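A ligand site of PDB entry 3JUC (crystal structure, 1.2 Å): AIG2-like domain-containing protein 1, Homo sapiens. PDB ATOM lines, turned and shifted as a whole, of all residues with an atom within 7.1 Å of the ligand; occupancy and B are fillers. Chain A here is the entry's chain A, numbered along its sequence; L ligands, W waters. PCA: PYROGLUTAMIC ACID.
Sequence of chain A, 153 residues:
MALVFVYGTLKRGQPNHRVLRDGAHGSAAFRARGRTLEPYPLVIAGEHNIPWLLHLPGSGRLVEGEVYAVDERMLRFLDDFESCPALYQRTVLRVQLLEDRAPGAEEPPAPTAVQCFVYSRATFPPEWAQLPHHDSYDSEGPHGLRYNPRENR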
ATOM      1  N   VAL A   4      -5.166   8.038 -26.895  1.00  0.00           N
ATOM      2  CA  VAL A   4      -4.937   6.768 -26.254  1.00  0.00           C
ATOM      3  C   VAL A   4      -4.445   7.031 -24.856  1.00  0.00           C
ATOM      4  O   VAL A   4      -3.525   7.849 -24.641  1.00  0.00           O
ATOM      5  CB  VAL A   4      -3.893   5.924 -27.048  1.00  0.00           C
ATOM      6  CG1 VAL A   4      -3.536   4.644 -26.299  1.00  0.00           C
ATOM      7  CG2 VAL A   4      -4.383   5.607 -28.479  1.00  0.00           C
ATOM      8  N   PHE A   5      -5.039   6.361 -23.889  1.00  0.00           N
ATOM      9  CA  PHE A   5      -4.626   6.360 -22.489  1.00  0.00           C
ATOM     10  C   PHE A   5      -3.707   5.164 -22.249  1.00  0.00           C
ATOM     11  O   PHE A   5      -4.169   4.023 -22.431  1.00  0.00           O
ATOM     12  CB  PHE A   5      -5.850   6.296 -21.566  1.00  0.00           C
ATOM     13  CG  PHE A   5      -5.539   6.219 -20.101  1.00  0.00           C
ATOM     14  CD1 PHE A   5      -5.101   7.353 -19.405  1.00  0.00           C
ATOM     15  CD2 PHE A   5      -5.719   5.054 -19.396  1.00  0.00           C
ATOM     16  CE1 PHE A   5      -4.878   7.271 -18.043  1.00  0.00           C
ATOM     17  CE2 PHE A   5      -5.472   4.990 -18.046  1.00  0.00           C
ATOM     18  CZ  PHE A   5      -5.075   6.103 -17.360  1.00  0.00           C
ATOM     19  N   VAL A   6      -2.466   5.417 -21.902  1.00  0.00           N
ATOM     20  CA  VAL A   6      -1.489   4.355 -21.642  1.00  0.00           C
ATOM     21  C   VAL A   6      -1.219   4.308 -20.139  1.00  0.00           C
ATOM     22  O   VAL A   6      -1.067   5.337 -19.474  1.00  0.00           O
ATOM     23  CB  VAL A   6      -0.214   4.463 -22.493  1.00  0.00           C
ATOM     24  CG1 VAL A   6      -0.550   4.397 -23.948  1.00  0.00           C
ATOM     25  CG2 VAL A   6       0.601   5.666 -22.164  1.00  0.00           C
ATOM     26  N   TYR A   7      -1.117   3.084 -19.628  1.00  0.00           N
ATOM     27  CA  TYR A   7      -1.023   2.829 -18.197  1.00  0.00           C
ATOM     28  C   TYR A   7       0.141   1.873 -17.835  1.00  0.00           C
ATOM     29  O   TYR A   7       0.382   1.671 -16.647  1.00  0.00           O
ATOM     30  CB  TYR A   7      -2.334   2.235 -17.654  1.00  0.00           C
ATOM     31  CG  TYR A   7      -2.683   0.937 -18.322  1.00  0.00           C
ATOM     32  CD1 TYR A   7      -2.107  -0.259 -17.914  1.00  0.00           C
ATOM     33  CD2 TYR A   7      -3.536   0.888 -19.415  1.00  0.00           C
ATOM     34  CE1 TYR A   7      -2.378  -1.485 -18.561  1.00  0.00           C
ATOM     35  CE2 TYR A   7      -3.812  -0.306 -20.081  1.00  0.00           C
ATOM     36  CZ  TYR A   7      -3.236  -1.487 -19.629  1.00  0.00           C
ATOM     37  OH  TYR A   7      -3.539  -2.701 -20.206  1.00  0.00           O
ATOM     38  N   GLY A   8       0.782   1.283 -18.825  1.00  0.00           N
ATOM     39  CA  GLY A   8       1.692   0.196 -18.608  1.00  0.00           C
ATOM     40  C   GLY A   8       3.081   0.509 -19.146  1.00  0.00           C
ATOM     41  O   GLY A   8       3.656   1.571 -18.853  1.00  0.00           O
ATOM     42  N   THR A   9       3.631  -0.421 -19.933  1.00  0.00           N
ATOM     43  CA  THR A   9       4.993  -0.307 -20.417  1.00  0.00           C
ATOM     44  C   THR A   9       5.222   0.805 -21.448  1.00  0.00           C
ATOM     45  O   THR A   9       6.355   1.126 -21.761  1.00  0.00           O
ATOM     46  CB  THR A   9       5.484  -1.648 -21.011  1.00  0.00           C
ATOM     47  OG1 THR A   9       4.774  -1.932 -22.193  1.00  0.00           O
ATOM     48  CG2 THR A   9       5.493  -2.785 -20.005  1.00  0.00           C
ATOM     49  N   LEU A  10       4.137   1.426 -21.955  1.00  0.00           N
ATOM     50  CA  LEU A  10       4.260   2.553 -22.883  1.00  0.00           C
ATOM     51  C   LEU A  10       4.452   3.912 -22.205  1.00  0.00           C
ATOM     52  O   LEU A  10       4.783   4.875 -22.919  1.00  0.00           O
ATOM     53  CB  LEU A  10       3.033   2.609 -23.806  1.00  0.00           C
ATOM     54  CG  LEU A  10       2.864   1.425 -24.805  1.00  0.00           C
ATOM     55  CD1 LEU A  10       1.462   1.493 -25.441  1.00  0.00           C
ATOM     56  CD2 LEU A  10       3.925   1.448 -25.875  1.00  0.00           C
ATOM     57  N   LYS A  11       4.219   4.017 -20.897  1.00  0.00           N
ATOM     58  CA  LYS A  11       4.357   5.303 -20.231  1.00  0.00           C
ATOM     59  C   LYS A  11       5.777   5.830 -20.279  1.00  0.00           C
ATOM     60  O   LYS A  11       6.736   5.067 -20.339  1.00  0.00           O
ATOM     61  CB  LYS A  11       3.950   5.183 -18.757  1.00  0.00           C
ATOM     62  CG  LYS A  11       2.460   4.932 -18.492  1.00  0.00           C
ATOM     63  CD  LYS A  11       2.108   5.069 -17.036  1.00  0.00           C
ATOM     64  CE  LYS A  11       2.868   4.134 -16.112  1.00  0.00           C
ATOM     65  NZ  LYS A  11       2.436   4.221 -14.714  1.00  0.00           N
ATOM     66  N   GLN A  14       9.034   3.926 -18.865  1.00  0.00           N
ATOM     67  CA  GLN A  14       8.748   2.496 -18.884  1.00  0.00           C
ATOM     68  C   GLN A  14       9.361   1.827 -20.108  1.00  0.00           C
ATOM     69  O   GLN A  14       9.707   2.479 -21.090  1.00  0.00           O
ATOM     70  CB  GLN A  14       7.240   2.243 -18.759  1.00  0.00           C
ATOM     71  CG  GLN A  14       6.678   2.710 -17.426  1.00  0.00           C
ATOM     72  CD  GLN A  14       7.349   2.013 -16.284  1.00  0.00           C
ATOM     73  OE1 GLN A  14       7.396   0.777 -16.275  1.00  0.00           O
ATOM     74  NE2 GLN A  14       7.839   2.758 -15.285  1.00  0.00           N
ATOM     75  N   ASN A  16       8.751   0.111 -22.872  1.00  0.00           N
ATOM     76  CA  ASN A  16       8.344   0.207 -24.269  1.00  0.00           C
ATOM     77  C   ASN A  16       7.977   1.591 -24.712  1.00  0.00           C
ATOM     78  O   ASN A  16       7.465   1.787 -25.817  1.00  0.00           O
ATOM     79  CB  ASN A  16       7.173  -0.751 -24.548  1.00  0.00           C
ATOM     80  CG  ASN A  16       7.555  -2.221 -24.491  1.00  0.00           C
ATOM     81  OD1 ASN A  16       6.764  -3.075 -23.984  1.00  0.00           O
ATOM     82  ND2 ASN A  16       8.673  -2.551 -25.047  1.00  0.00           N
ATOM     83  N   LEU A  42      -5.789  -3.523 -12.280  1.00  0.00           N
ATOM     84  CA  LEU A  42      -4.580  -3.493 -13.060  1.00  0.00           C
ATOM     85  C   LEU A  42      -3.603  -4.433 -12.339  1.00  0.00           C
ATOM     86  O   LEU A  42      -3.240  -4.187 -11.182  1.00  0.00           O
ATOM     87  CB  LEU A  42      -4.019  -2.060 -13.136  1.00  0.00           C
ATOM     88  CG  LEU A  42      -2.620  -1.922 -13.744  1.00  0.00           C
ATOM     89  CD1 LEU A  42      -2.540  -2.506 -15.158  1.00  0.00           C
ATOM     90  CD2 LEU A  42      -2.185  -0.439 -13.733  1.00  0.00           C
ATOM     91  N   ILE A  50       3.924  -8.837 -17.528  1.00  0.00           N
ATOM     92  CA  ILE A  50       3.213  -7.801 -18.246  1.00  0.00           C
ATOM     93  C   ILE A  50       2.073  -7.238 -17.397  1.00  0.00           C
ATOM     94  O   ILE A  50       1.406  -7.979 -16.675  1.00  0.00           O
ATOM     95  CB  ILE A  50       2.641  -8.469 -19.553  1.00  0.00           C
ATOM     96  CG1 ILE A  50       3.780  -8.721 -20.564  1.00  0.00           C
ATOM     97  CG2 ILE A  50       1.543  -7.611 -20.185  1.00  0.00           C
ATOM     98  CD1 ILE A  50       3.419  -9.680 -21.670  1.00  0.00           C
ATOM     99  N   PRO A  51       1.830  -5.932 -17.485  1.00  0.00           N
ATOM    100  CA  PRO A  51       0.651  -5.331 -16.855  1.00  0.00           C
ATOM    101  C   PRO A  51      -0.606  -5.445 -17.724  1.00  0.00           C
ATOM    102  O   PRO A  51      -0.556  -5.202 -18.932  1.00  0.00           O
ATOM    103  CB  PRO A  51       1.081  -3.875 -16.653  1.00  0.00           C
ATOM    104  CG  PRO A  51       1.965  -3.602 -17.846  1.00  0.00           C
ATOM    105  CD  PRO A  51       2.705  -4.904 -18.079  1.00  0.00           C
ATOM    106  N   TRP A  52      -1.701  -5.828 -17.078  1.00  0.00           N
ATOM    107  CA  TRP A  52      -2.976  -6.039 -17.767  1.00  0.00           C
ATOM    108  C   TRP A  52      -4.067  -5.253 -17.047  1.00  0.00           C
ATOM    109  O   TRP A  52      -4.323  -5.465 -15.858  1.00  0.00           O
ATOM    110  CB  TRP A  52      -3.371  -7.530 -17.737  1.00  0.00           C
ATOM    111  CG  TRP A  52      -2.325  -8.504 -18.117  1.00  0.00           C
ATOM    112  CD1 TRP A  52      -1.452  -9.126 -17.257  1.00  0.00           C
ATOM    113  CD2 TRP A  52      -1.971  -8.988 -19.418  1.00  0.00           C
ATOM    114  NE1 TRP A  52      -0.620  -9.962 -17.926  1.00  0.00           N
ATOM    115  CE2 TRP A  52      -0.917  -9.924 -19.251  1.00  0.00           C
ATOM    116  CE3 TRP A  52      -2.451  -8.750 -20.708  1.00  0.00           C
ATOM    117  CZ2 TRP A  52      -0.307 -10.556 -20.322  1.00  0.00           C
ATOM    118  CZ3 TRP A  52      -1.801  -9.396 -21.791  1.00  0.00           C
ATOM    119  CH2 TRP A  52      -0.777 -10.320 -21.584  1.00  0.00           C
ATOM    120  N   LEU A  53      -4.722  -4.350 -17.805  1.00  0.00           N
ATOM    121  CA  LEU A  53      -5.944  -3.660 -17.315  1.00  0.00           C
ATOM    122  C   LEU A  53      -7.097  -4.596 -17.592  1.00  0.00           C
ATOM    123  O   LEU A  53      -7.570  -4.710 -18.739  1.00  0.00           O
ATOM    124  CB  LEU A  53      -6.112  -2.318 -18.005  1.00  0.00           C
ATOM    125  CG  LEU A  53      -7.179  -1.451 -17.404  1.00  0.00           C
ATOM    126  CD1 LEU A  53      -6.665  -0.827 -16.109  1.00  0.00           C
ATOM    127  CD2 LEU A  53      -7.651  -0.373 -18.367  1.00  0.00           C
ATOM    128  N   PHE A  81       1.132  -4.109 -31.911  1.00  0.00           N
ATOM    129  CA  PHE A  81       2.062  -4.168 -30.785  1.00  0.00           C
ATOM    130  C   PHE A  81       1.422  -4.837 -29.571  1.00  0.00           C
ATOM    131  O   PHE A  81       2.099  -5.591 -28.857  1.00  0.00           O
ATOM    132  CB  PHE A  81       2.558  -2.755 -30.468  1.00  0.00           C
ATOM    133  CG  PHE A  81       3.733  -2.728 -29.486  1.00  0.00           C
ATOM    134  CD1 PHE A  81       4.997  -3.003 -29.920  1.00  0.00           C
ATOM    135  CD2 PHE A  81       3.584  -2.309 -28.190  1.00  0.00           C
ATOM    136  CE1 PHE A  81       6.098  -3.007 -29.075  1.00  0.00           C
ATOM    137  CE2 PHE A  81       4.691  -2.312 -27.304  1.00  0.00           C
ATOM    138  CZ  PHE A  81       5.928  -2.644 -27.774  1.00  0.00           C
ATOM    139  N   GLU A  82       0.149  -4.603 -29.372  1.00  0.00           N
ATOM    140  CA  GLU A  82      -0.632  -5.179 -28.275  1.00  0.00           C
ATOM    141  C   GLU A  82      -1.410  -6.470 -28.669  1.00  0.00           C
ATOM    142  O   GLU A  82      -2.286  -6.971 -27.932  1.00  0.00           O
ATOM    143  CB  GLU A  82      -1.589  -4.136 -27.682  1.00  0.00           C
ATOM    144  CG  GLU A  82      -0.851  -2.904 -27.157  1.00  0.00           C
ATOM    145  CD  GLU A  82       0.200  -3.188 -26.021  1.00  0.00           C
ATOM    146  OE1 GLU A  82       0.162  -4.199 -25.384  1.00  0.00           O
ATOM    147  OE2 GLU A  82       1.157  -2.369 -25.847  1.00  0.00           O
ATOM    148  N   TYR A  88      -5.086  -8.253 -26.036  1.00  0.00           N
ATOM    149  CA  TYR A  88      -5.802  -7.060 -25.564  1.00  0.00           C
ATOM    150  C   TYR A  88      -6.875  -6.729 -26.595  1.00  0.00           C
ATOM    151  O   TYR A  88      -6.770  -7.113 -27.768  1.00  0.00           O
ATOM    152  CB  TYR A  88      -4.872  -5.847 -25.411  1.00  0.00           C
ATOM    153  CG  TYR A  88      -3.779  -5.951 -24.357  1.00  0.00           C
ATOM    154  CD1 TYR A  88      -3.964  -5.409 -23.091  1.00  0.00           C
ATOM    155  CD2 TYR A  88      -2.543  -6.539 -24.633  1.00  0.00           C
ATOM    156  CE1 TYR A  88      -2.937  -5.425 -22.139  1.00  0.00           C
ATOM    157  CE2 TYR A  88      -1.513  -6.556 -23.711  1.00  0.00           C
ATOM    158  CZ  TYR A  88      -1.720  -5.987 -22.467  1.00  0.00           C
ATOM    159  OH  TYR A  88      -0.650  -5.997 -21.579  1.00  0.00           O
ATOM    160  N   VAL A 118      -8.141   2.650 -24.835  1.00  0.00           N
ATOM    161  CA  VAL A 118      -7.256   1.977 -23.896  1.00  0.00           C
ATOM    162  C   VAL A 118      -7.149   0.535 -24.350  1.00  0.00           C
ATOM    163  O   VAL A 118      -8.078  -0.022 -24.951  1.00  0.00           O
ATOM    164  CB  VAL A 118      -7.798   2.047 -22.435  1.00  0.00           C
ATOM    165  CG1 VAL A 118      -9.101   1.210 -22.273  1.00  0.00           C
ATOM    166  CG2 VAL A 118      -6.757   1.669 -21.390  1.00  0.00           C
ATOM    167  N   TYR A 119      -6.025  -0.131 -24.043  1.00  0.00           N
ATOM    168  CA  TYR A 119      -5.850  -1.550 -24.290  1.00  0.00           C
ATOM    169  C   TYR A 119      -6.186  -2.322 -23.010  1.00  0.00           C
ATOM    170  O   TYR A 119      -5.463  -2.279 -22.020  1.00  0.00           O
ATOM    171  CB  TYR A 119      -4.416  -1.838 -24.787  1.00  0.00           C
ATOM    172  CG  TYR A 119      -4.205  -1.270 -26.144  1.00  0.00           C
ATOM    173  CD1 TYR A 119      -4.725  -1.901 -27.268  1.00  0.00           C
ATOM    174  CD2 TYR A 119      -3.529  -0.048 -26.326  1.00  0.00           C
ATOM    175  CE1 TYR A 119      -4.587  -1.342 -28.565  1.00  0.00           C
ATOM    176  CE2 TYR A 119      -3.387   0.486 -27.569  1.00  0.00           C
ATOM    177  CZ  TYR A 119      -3.905  -0.138 -28.686  1.00  0.00           C
ATOM    178  OH  TYR A 119      -3.760   0.447 -29.909  1.00  0.00           O
ATOM    179  N   SER A 120      -7.350  -2.977 -23.017  1.00  0.00           N
ATOM    180  CA  SER A 120      -7.837  -3.728 -21.864  1.00  0.00           C
ATOM    181  C   SER A 120      -7.890  -5.221 -22.220  1.00  0.00           C
ATOM    182  O   SER A 120      -7.661  -5.605 -23.384  1.00  0.00           O
ATOM    183  CB  SER A 120      -9.183  -3.198 -21.438  1.00  0.00           C
ATOM    184  OG  SER A 120     -10.155  -3.294 -22.449  1.00  0.00           O
ATOM    185  N   TYR A 137       1.462   1.644 -12.479  1.00  0.00           N
ATOM    186  CA  TYR A 137       2.412   0.603 -12.865  1.00  0.00           C
ATOM    187  C   TYR A 137       3.820   1.166 -13.035  1.00  0.00           C
ATOM    188  O   TYR A 137       4.012   2.200 -13.680  1.00  0.00           O
ATOM    189  CB  TYR A 137       1.953  -0.063 -14.190  1.00  0.00           C
ATOM    190  CG  TYR A 137       3.018  -0.966 -14.767  1.00  0.00           C
ATOM    191  CD1 TYR A 137       3.267  -2.225 -14.261  1.00  0.00           C
ATOM    192  CD2 TYR A 137       3.849  -0.517 -15.790  1.00  0.00           C
ATOM    193  CE1 TYR A 137       4.254  -3.043 -14.757  1.00  0.00           C
ATOM    194  CE2 TYR A 137       4.863  -1.320 -16.310  1.00  0.00           C
ATOM    195  CZ  TYR A 137       5.070  -2.583 -15.788  1.00  0.00           C
ATOM    196  OH  TYR A 137       6.068  -3.344 -16.317  1.00  0.00           O
ATOM    197  N   TYR A 147       9.483  -6.189 -15.866  1.00  0.00           N
ATOM    198  CA  TYR A 147       9.051  -6.604 -17.195  1.00  0.00           C
ATOM    199  C   TYR A 147      10.153  -7.275 -17.892  1.00  0.00           C
ATOM    200  O   TYR A 147      11.295  -6.793 -17.874  1.00  0.00           O
ATOM    201  CB  TYR A 147       8.588  -5.392 -17.961  1.00  0.00           C
ATOM    202  CG  TYR A 147       8.301  -5.605 -19.439  1.00  0.00           C
ATOM    203  CD1 TYR A 147       7.238  -6.367 -19.863  1.00  0.00           C
ATOM    204  CD2 TYR A 147       9.091  -5.028 -20.407  1.00  0.00           C
ATOM    205  CE1 TYR A 147       7.017  -6.522 -21.228  1.00  0.00           C
ATOM    206  CE2 TYR A 147       8.844  -5.192 -21.741  1.00  0.00           C
ATOM    207  CZ  TYR A 147       7.789  -5.916 -22.148  1.00  0.00           C
ATOM    208  OH  TYR A 147       7.534  -6.062 -23.514  1.00  0.00           O
HETATM  209  N   PCA L   1       1.326  -1.421 -22.749  1.00  0.00           N
HETATM  210  CA  PCA L   1       0.052  -0.729 -22.864  1.00  0.00           C
HETATM  211  CB  PCA L   1      -0.971  -1.825 -22.335  1.00  0.00           C
HETATM  212  CG  PCA L   1      -0.169  -2.489 -21.220  1.00  0.00           C
HETATM  213  CD  PCA L   1       1.279  -2.291 -21.682  1.00  0.00           C
HETATM  214  OE  PCA L   1       2.290  -2.797 -21.202  1.00  0.00           O
HETATM  215  C   PCA L   1       0.018   0.529 -22.048  1.00  0.00           C
HETATM  216  O   PCA L   1      -1.073   1.053 -21.863  1.00  0.00           O
HETATM  217  OXT PCA L   1       1.108   0.986 -21.593  1.00  0.00           O
HETATM  218  O   HOH W   1      -3.655   1.374 -23.125  1.00  0.00           O
HETATM  219  O   HOH W   2       1.525  -5.390 -23.259  1.00  0.00           O
HETATM  220  O   HOH W   3       3.224  -3.371 -24.512  1.00  0.00           O
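Val 6 touches the ligand. CG of Pro 51 touches OE of the ligand, at 3.5 Å. Tyr 88 touches the ligand. Within 4 Å of the ligand: Val 6, Tyr 7, Gly 8, Thr 9, Leu 10, Pro 51, Glu 82 and Tyr 88. The nearest printed residue that does not touch the ligand is Tyr 119 (4.2 Å).
The side-chain hydroxyl of Tyr 7 lies within hydrogen-bond range of the backbone NH of Leu 53, 3.1 Å away. O of Tyr 119 is in hydrogen-bond range of OH of Tyr 7, at 2.7 Å. O of Pro 51 sits at hydrogen-bond distance from OH of Tyr 88 (2.8 Å). O of Thr 9 sits at hydrogen-bond distance from N of Asn 16.
Water W1 lies within hydrogen-bond range of the backbone carbonyl oxygen (O) of Phe 5 (2.8 Å), an oxygen (O) of the ligand (2.9 Å) and the backbone NH (N) of Tyr 119 (3.0 Å). Water W3 lies within hydrogen-bond range of the side-chain carboxylate of Glu 82 (2.7 Å), the side-chain hydroxyl of Thr 9 (3.1 Å) and a nitrogen (N) of the ligand (3.2 Å). Water W2 lies within hydrogen-bond range of OE1 of Glu 82, OH of Tyr 88 and OE of the ligand.
N of Gly 8 is in hydrogen-bond range of OXT of the ligand. An oxygen (OXT) of the ligand is in hydrogen-bond range of the backbone NH of Leu 10. The side-chain carboxylate (OE2) of Glu 82 lies within hydrogen-bond range of a nitrogen (N) of the ligand, at 3.2 Å. The backbone NH (N) of Tyr 7 sits at hydrogen-bond distance from an oxygen (O) of the ligand (3.0 Å). The backbone NH (N) of Thr 9 is in hydrogen-bond range of an oxygen (OE) of the ligand (3.0 Å). OG1 of Thr 9 sits at hydrogen-bond distance from OE of the ligand, 2.8 Å away.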
